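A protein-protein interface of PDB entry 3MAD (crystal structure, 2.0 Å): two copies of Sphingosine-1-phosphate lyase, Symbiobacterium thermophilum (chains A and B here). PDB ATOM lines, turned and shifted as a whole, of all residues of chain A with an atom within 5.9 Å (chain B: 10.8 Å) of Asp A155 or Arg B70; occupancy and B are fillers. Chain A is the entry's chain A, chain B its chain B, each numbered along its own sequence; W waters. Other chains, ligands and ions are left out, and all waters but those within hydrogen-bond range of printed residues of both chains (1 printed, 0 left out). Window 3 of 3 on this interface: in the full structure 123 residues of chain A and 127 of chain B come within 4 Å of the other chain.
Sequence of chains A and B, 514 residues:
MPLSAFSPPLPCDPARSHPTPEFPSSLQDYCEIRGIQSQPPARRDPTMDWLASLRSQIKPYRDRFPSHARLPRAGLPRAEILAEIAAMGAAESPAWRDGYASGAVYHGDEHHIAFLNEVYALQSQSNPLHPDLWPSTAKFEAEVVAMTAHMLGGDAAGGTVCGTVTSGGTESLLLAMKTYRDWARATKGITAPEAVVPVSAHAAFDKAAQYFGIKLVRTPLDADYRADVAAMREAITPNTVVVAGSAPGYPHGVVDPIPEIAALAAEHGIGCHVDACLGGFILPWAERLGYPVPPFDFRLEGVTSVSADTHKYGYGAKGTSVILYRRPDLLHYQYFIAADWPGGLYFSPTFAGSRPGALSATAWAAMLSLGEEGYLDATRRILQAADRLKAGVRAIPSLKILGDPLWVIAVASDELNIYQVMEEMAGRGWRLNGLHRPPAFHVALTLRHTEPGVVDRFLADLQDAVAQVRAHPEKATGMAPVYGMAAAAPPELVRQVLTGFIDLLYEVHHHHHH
O of Leu A368 lies within hydrogen-bond range of N of Leu B76 (2.8 Å). The side-chain carboxylate (OD1) of Asp A155 is in salt-bridge range of the guanidinium group (NH2) of Arg B70. The backbone carbonyl oxygen of Arg B70 lies close to the side-chain sulfur of Met A147, at 3.7 Å. O of Ala B69 lies close to O of Ala A146, at 3.3 Å. A ring nitrogen (NE2) of His A150 sits at hydrogen-bond distance from the guanidinium group (NE) of Arg B70.
Among the printed residues, merely in contact across the chains: Leu A368 with Gly B75, Met A147 with Ala B69, Met A147 with His B68, Leu A368 with Pro B72, Leu A368 with His B68, Ala A146 with Val B508 and Met A147 with Leu B71.
Asp A155 touches just one residue of chain B: Arg B70 (2.7 Å). Arg B70 touches just these residues of chain A: Met A147 (3.6 Å), His A150 (3.3 Å) and Asp A155 (2.7 Å). Of the printed residues of chain B, Met A147 touches His B68 (3.7 Å), Ala B69 (3.6 Å), Arg B70 (3.6 Å) and Leu B71 (3.9 Å). His A150 touches one residue of chain B. No residue of chain B comes within 4 Å of Gly A154. No residue of chain B comes within 4 Å of Ala A157. No residue of chain B comes within 4 Å of Gly A158. Printed residues of chain A within 4 Å of Gly B75: Leu A368. Of the printed residues of chain B, Leu A368 touches His B68, Pro B72, Gly B75 and Leu B76. Of the printed residues of chain A, His B68 touches Met A147 and Leu A368. Of the printed residues of chain B, Ala A146 touches Ala B69 (3.3 Å) and Val B508 (3.8 Å). Ala A149 touches none of the printed residues of chain B. Ala B74 touches none of the printed residues of chain A. The nearest residue of chain B that does not touch Asp A155 is Ala B69 (6.7 Å). The nearest residue of chain A that does not touch Arg B70 is Ala A146 (5.2 Å). The nearest printed residue of chain A that does not touch Leu B76 is Met A147 (7.8 Å).
Of the 12 printed residues of chain B, 8 touch a printed residue of chain A. Hydrophobic or aromatic side chains of chain B that line the printed part of chain A: His B68, Leu B71, Pro B72, Leu B76 and Val B508. Among the printed residues, 12 pairs touch across the chains.
No position is printed for both chains. Of the 12 pairs that touch across the chains among the printed residues, none has its exchanged pair printed and touching as well.
Water W1 lies within hydrogen-bond range of the backbone NH (N) of Leu B71 (2.8 Å), the backbone carbonyl oxygen (O) of Met A147 (2.8 Å) and a ring nitrogen (ND1) of His A150 (3.0 Å).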
ATOM      1  N   ALA A 146      29.432  -8.814 -27.810  1.00  0.00           N
ATOM      2  CA  ALA A 146      28.263  -9.657 -27.540  1.00  0.00           C
ATOM      3  C   ALA A 146      27.465  -9.194 -26.328  1.00  0.00           C
ATOM      4  O   ALA A 146      26.237  -9.120 -26.375  1.00  0.00           O
ATOM      5  CB  ALA A 146      28.690 -11.127 -27.362  1.00  0.00           C
ATOM      6  N   MET A 147      28.169  -8.920 -25.232  1.00  0.00           N
ATOM      7  CA  MET A 147      27.533  -8.484 -23.999  1.00  0.00           C
ATOM      8  C   MET A 147      26.856  -7.131 -24.192  1.00  0.00           C
ATOM      9  O   MET A 147      25.733  -6.903 -23.731  1.00  0.00           O
ATOM     10  CB  MET A 147      28.567  -8.413 -22.866  1.00  0.00           C
ATOM     11  CG  MET A 147      29.187  -9.765 -22.521  1.00  0.00           C
ATOM     12  SD  MET A 147      30.128  -9.787 -20.978  1.00  0.00           S
ATOM     13  CE  MET A 147      31.653  -8.949 -21.435  1.00  0.00           C
ATOM     14  N   ALA A 149      25.807  -5.850 -27.075  1.00  0.00           N
ATOM     15  CA  ALA A 149      24.674  -6.021 -27.983  1.00  0.00           C
ATOM     16  C   ALA A 149      23.455  -6.530 -27.218  1.00  0.00           C
ATOM     17  O   ALA A 149      22.336  -6.063 -27.420  1.00  0.00           O
ATOM     18  CB  ALA A 149      25.031  -6.986 -29.107  1.00  0.00           C
ATOM     19  N   HIS A 150      23.674  -7.492 -26.336  1.00  0.00           N
ATOM     20  CA  HIS A 150      22.579  -8.027 -25.541  1.00  0.00           C
ATOM     21  C   HIS A 150      21.981  -6.958 -24.625  1.00  0.00           C
ATOM     22  O   HIS A 150      20.766  -6.843 -24.512  1.00  0.00           O
ATOM     23  CB  HIS A 150      23.039  -9.221 -24.709  1.00  0.00           C
ATOM     24  CG  HIS A 150      22.003  -9.703 -23.747  1.00  0.00           C
ATOM     25  ND1 HIS A 150      22.056  -9.429 -22.395  1.00  0.00           N
ATOM     26  CD2 HIS A 150      20.871 -10.419 -23.944  1.00  0.00           C
ATOM     27  CE1 HIS A 150      21.005  -9.968 -21.800  1.00  0.00           C
ATOM     28  NE2 HIS A 150      20.269 -10.572 -22.717  1.00  0.00           N
ATOM     29  N   GLY A 153      19.432  -4.639 -26.405  1.00  0.00           N
ATOM     30  CA  GLY A 153      18.253  -5.185 -27.064  1.00  0.00           C
ATOM     31  C   GLY A 153      18.501  -5.977 -28.338  1.00  0.00           C
ATOM     32  O   GLY A 153      17.582  -6.189 -29.131  1.00  0.00           O
ATOM     33  N   GLY A 154      19.737  -6.422 -28.537  1.00  0.00           N
ATOM     34  CA  GLY A 154      20.090  -7.200 -29.713  1.00  0.00           C
ATOM     35  C   GLY A 154      19.255  -8.453 -29.914  1.00  0.00           C
ATOM     36  O   GLY A 154      18.922  -8.797 -31.047  1.00  0.00           O
ATOM     37  N   ASP A 155      18.921  -9.140 -28.825  1.00  0.00           N
ATOM     38  CA  ASP A 155      18.080 -10.336 -28.903  1.00  0.00           C
ATOM     39  C   ASP A 155      16.730 -10.029 -29.553  1.00  0.00           C
ATOM     40  O   ASP A 155      16.119 -10.901 -30.173  1.00  0.00           O
ATOM     41  CB  ASP A 155      17.858 -10.950 -27.517  1.00  0.00           C
ATOM     42  CG  ASP A 155      19.046 -11.770 -27.038  1.00  0.00           C
ATOM     43  OD1 ASP A 155      18.857 -12.591 -26.118  1.00  0.00           O
ATOM     44  OD2 ASP A 155      20.165 -11.604 -27.578  1.00  0.00           O
ATOM     45  N   ALA A 156      16.267  -8.791 -29.407  1.00  0.00           N
ATOM     46  CA  ALA A 156      15.014  -8.364 -30.033  1.00  0.00           C
ATOM     47  C   ALA A 156      15.143  -8.260 -31.551  1.00  0.00           C
ATOM     48  O   ALA A 156      14.142  -8.223 -32.260  1.00  0.00           O
ATOM     49  CB  ALA A 156      14.539  -7.039 -29.444  1.00  0.00           C
ATOM     50  N   ALA A 157      16.378  -8.223 -32.045  1.00  0.00           N
ATOM     51  CA  ALA A 157      16.622  -8.156 -33.480  1.00  0.00           C
ATOM     52  C   ALA A 157      16.692  -9.549 -34.093  1.00  0.00           C
ATOM     53  O   ALA A 157      16.812  -9.697 -35.310  1.00  0.00           O
ATOM     54  CB  ALA A 157      17.898  -7.381 -33.769  1.00  0.00           C
ATOM     55  N   GLY A 158      16.624 -10.569 -33.243  1.00  0.00           N
ATOM     56  CA  GLY A 158      16.610 -11.946 -33.698  1.00  0.00           C
ATOM     57  C   GLY A 158      17.974 -12.608 -33.690  1.00  0.00           C
ATOM     58  O   GLY A 158      18.147 -13.697 -34.234  1.00  0.00           O
ATOM     59  N   GLY A 159      18.948 -11.947 -33.078  1.00  0.00           N
ATOM     60  CA  GLY A 159      20.286 -12.499 -32.976  1.00  0.00           C
ATOM     61  C   GLY A 159      21.159 -12.209 -34.182  1.00  0.00           C
ATOM     62  O   GLY A 159      22.172 -12.874 -34.397  1.00  0.00           O
ATOM     63  N   VAL A 161      22.302  -9.044 -34.561  1.00  0.00           N
ATOM     64  CA  VAL A 161      23.108  -7.899 -34.148  1.00  0.00           C
ATOM     65  C   VAL A 161      24.576  -8.290 -34.001  1.00  0.00           C
ATOM     66  O   VAL A 161      24.903  -9.331 -33.426  1.00  0.00           O
ATOM     67  CB  VAL A 161      22.610  -7.272 -32.836  1.00  0.00           C
ATOM     68  CG1 VAL A 161      23.559  -6.182 -32.385  1.00  0.00           C
ATOM     69  CG2 VAL A 161      21.203  -6.707 -33.012  1.00  0.00           C
ATOM     70  N   LEU A 368      32.873  -7.441 -16.841  1.00  0.00           N
ATOM     71  CA  LEU A 368      32.754  -8.662 -16.039  1.00  0.00           C
ATOM     72  C   LEU A 368      32.804  -8.408 -14.528  1.00  0.00           C
ATOM     73  O   LEU A 368      32.076  -9.043 -13.771  1.00  0.00           O
ATOM     74  CB  LEU A 368      33.831  -9.676 -16.432  1.00  0.00           C
ATOM     75  CG  LEU A 368      33.725 -10.290 -17.829  1.00  0.00           C
ATOM     76  CD1 LEU A 368      34.791 -11.361 -18.014  1.00  0.00           C
ATOM     77  CD2 LEU A 368      32.344 -10.872 -18.037  1.00  0.00           C
ATOM     78  N   PRO B  66      35.211 -19.964 -19.491  1.00  0.00           N
ATOM     79  CA  PRO B  66      33.816 -19.681 -19.834  1.00  0.00           C
ATOM     80  C   PRO B  66      33.741 -18.586 -20.893  1.00  0.00           C
ATOM     81  O   PRO B  66      34.550 -17.660 -20.869  1.00  0.00           O
ATOM     82  CB  PRO B  66      33.233 -19.174 -18.507  1.00  0.00           C
ATOM     83  CG  PRO B  66      34.428 -18.694 -17.737  1.00  0.00           C
ATOM     84  CD  PRO B  66      35.481 -19.702 -18.068  1.00  0.00           C
ATOM     85  N   SER B  67      32.805 -18.705 -21.827  1.00  0.00           N
ATOM     86  CA  SER B  67      32.586 -17.650 -22.807  1.00  0.00           C
ATOM     87  C   SER B  67      31.451 -16.751 -22.316  1.00  0.00           C
ATOM     88  O   SER B  67      30.508 -17.229 -21.688  1.00  0.00           O
ATOM     89  CB  SER B  67      32.275 -18.241 -24.185  1.00  0.00           C
ATOM     90  OG  SER B  67      31.112 -19.050 -24.139  1.00  0.00           O
ATOM     91  N   HIS B  68      31.549 -15.452 -22.585  1.00  0.00           N
ATOM     92  CA  HIS B  68      30.572 -14.502 -22.060  1.00  0.00           C
ATOM     93  C   HIS B  68      29.797 -13.811 -23.175  1.00  0.00           C
ATOM     94  O   HIS B  68      30.331 -12.956 -23.886  1.00  0.00           O
ATOM     95  CB  HIS B  68      31.258 -13.469 -21.157  1.00  0.00           C
ATOM     96  CG  HIS B  68      32.013 -14.074 -20.013  1.00  0.00           C
ATOM     97  ND1 HIS B  68      31.402 -14.455 -18.838  1.00  0.00           N
ATOM     98  CD2 HIS B  68      33.326 -14.373 -19.869  1.00  0.00           C
ATOM     99  CE1 HIS B  68      32.305 -14.964 -18.020  1.00  0.00           C
ATOM    100  NE2 HIS B  68      33.482 -14.921 -18.617  1.00  0.00           N
ATOM    101  N   ALA B  69      28.536 -14.195 -23.334  1.00  0.00           N
ATOM    102  CA  ALA B  69      27.702 -13.625 -24.380  1.00  0.00           C
ATOM    103  C   ALA B  69      26.748 -12.596 -23.783  1.00  0.00           C
ATOM    104  O   ALA B  69      26.121 -11.830 -24.505  1.00  0.00           O
ATOM    105  CB  ALA B  69      26.926 -14.722 -25.109  1.00  0.00           C
ATOM    106  N   ARG B  70      26.653 -12.584 -22.457  1.00  0.00           N
ATOM    107  CA  ARG B  70      25.811 -11.636 -21.745  1.00  0.00           C
ATOM    108  C   ARG B  70      26.535 -11.202 -20.484  1.00  0.00           C
ATOM    109  O   ARG B  70      27.360 -11.946 -19.949  1.00  0.00           O
ATOM    110  CB  ARG B  70      24.470 -12.279 -21.368  1.00  0.00           C
ATOM    111  CG  ARG B  70      23.639 -12.734 -22.565  1.00  0.00           C
ATOM    112  CD  ARG B  70      22.354 -13.459 -22.142  1.00  0.00           C
ATOM    113  NE  ARG B  70      21.454 -13.642 -23.285  1.00  0.00           N
ATOM    114  CZ  ARG B  70      20.417 -14.477 -23.313  1.00  0.00           C
ATOM    115  NH1 ARG B  70      20.132 -15.231 -22.259  1.00  0.00           N
ATOM    116  NH2 ARG B  70      19.666 -14.564 -24.406  1.00  0.00           N
ATOM    117  N   LEU B  71      26.242  -9.995 -20.018  1.00  0.00           N
ATOM    118  CA  LEU B  71      26.753  -9.544 -18.732  1.00  0.00           C
ATOM    119  C   LEU B  71      26.417 -10.583 -17.673  1.00  0.00           C
ATOM    120  O   LEU B  71      25.300 -11.100 -17.653  1.00  0.00           O
ATOM    121  CB  LEU B  71      26.092  -8.230 -18.340  1.00  0.00           C
ATOM    122  CG  LEU B  71      26.905  -6.935 -18.232  1.00  0.00           C
ATOM    123  CD1 LEU B  71      28.294  -7.040 -18.837  1.00  0.00           C
ATOM    124  CD2 LEU B  71      26.121  -5.761 -18.808  1.00  0.00           C
ATOM    125  N   PRO B  72      27.377 -10.885 -16.783  1.00  0.00           N
ATOM    126  CA  PRO B  72      27.057 -11.753 -15.650  1.00  0.00           C
ATOM    127  C   PRO B  72      26.029 -11.033 -14.797  1.00  0.00           C
ATOM    128  O   PRO B  72      26.016  -9.814 -14.797  1.00  0.00           O
ATOM    129  CB  PRO B  72      28.385 -11.853 -14.899  1.00  0.00           C
ATOM    130  CG  PRO B  72      29.428 -11.425 -15.867  1.00  0.00           C
ATOM    131  CD  PRO B  72      28.774 -10.422 -16.754  1.00  0.00           C
ATOM    132  N   ARG B  73      25.170 -11.762 -14.098  1.00  0.00           N
ATOM    133  CA  ARG B  73      24.163 -11.125 -13.259  1.00  0.00           C
ATOM    134  C   ARG B  73      24.843 -10.370 -12.114  1.00  0.00           C
ATOM    135  O   ARG B  73      24.572  -9.192 -11.894  1.00  0.00           O
ATOM    136  CB  ARG B  73      23.182 -12.167 -12.723  1.00  0.00           C
ATOM    137  CG  ARG B  73      21.757 -11.658 -12.537  1.00  0.00           C
ATOM    138  CD  ARG B  73      21.628 -10.767 -11.311  1.00  0.00           C
ATOM    139  NE  ARG B  73      22.345 -11.316 -10.161  1.00  0.00           N
ATOM    140  CZ  ARG B  73      21.952 -12.379  -9.463  1.00  0.00           C
ATOM    141  NH1 ARG B  73      20.839 -13.022  -9.800  1.00  0.00           N
ATOM    142  NH2 ARG B  73      22.675 -12.803  -8.430  1.00  0.00           N
ATOM    143  N   ALA B  74      25.731 -11.054 -11.399  1.00  0.00           N
ATOM    144  CA  ALA B  74      26.549 -10.425 -10.367  1.00  0.00           C
ATOM    145  C   ALA B  74      27.964 -10.242 -10.906  1.00  0.00           C
ATOM    146  O   ALA B  74      28.421 -11.031 -11.728  1.00  0.00           O
ATOM    147  CB  ALA B  74      26.571 -11.278  -9.099  1.00  0.00           C
ATOM    148  N   GLY B  75      28.650  -9.197 -10.461  1.00  0.00           N
ATOM    149  CA  GLY B  75      30.013  -8.963 -10.898  1.00  0.00           C
ATOM    150  C   GLY B  75      30.902 -10.131 -10.517  1.00  0.00           C
ATOM    151  O   GLY B  75      30.740 -10.709  -9.451  1.00  0.00           O
ATOM    152  N   LEU B  76      31.833 -10.493 -11.391  1.00  0.00           N
ATOM    153  CA  LEU B  76      32.764 -11.559 -11.073  1.00  0.00           C
ATOM    154  C   LEU B  76      33.948 -10.988 -10.296  1.00  0.00           C
ATOM    155  O   LEU B  76      34.293  -9.811 -10.450  1.00  0.00           O
ATOM    156  CB  LEU B  76      33.232 -12.268 -12.346  1.00  0.00           C
ATOM    157  CG  LEU B  76      32.135 -12.939 -13.181  1.00  0.00           C
ATOM    158  CD1 LEU B  76      32.670 -13.342 -14.538  1.00  0.00           C
ATOM    159  CD2 LEU B  76      31.527 -14.139 -12.450  1.00  0.00           C
ATOM    160  N   VAL B 508      30.898 -15.772 -30.624  1.00  0.00           N
ATOM    161  CA  VAL B 508      30.970 -16.167 -29.218  1.00  0.00           C
ATOM    162  C   VAL B 508      30.247 -17.493 -28.977  1.00  0.00           C
ATOM    163  O   VAL B 508      30.815 -18.444 -28.436  1.00  0.00           O
ATOM    164  CB  VAL B 508      30.369 -15.096 -28.284  1.00  0.00           C
ATOM    165  CG1 VAL B 508      30.356 -15.604 -26.855  1.00  0.00           C
ATOM    166  CG2 VAL B 508      31.158 -13.809 -28.380  1.00  0.00           C
HETATM  167  O   HOH W   1      24.678  -8.198 -21.453  1.00  0.00           O
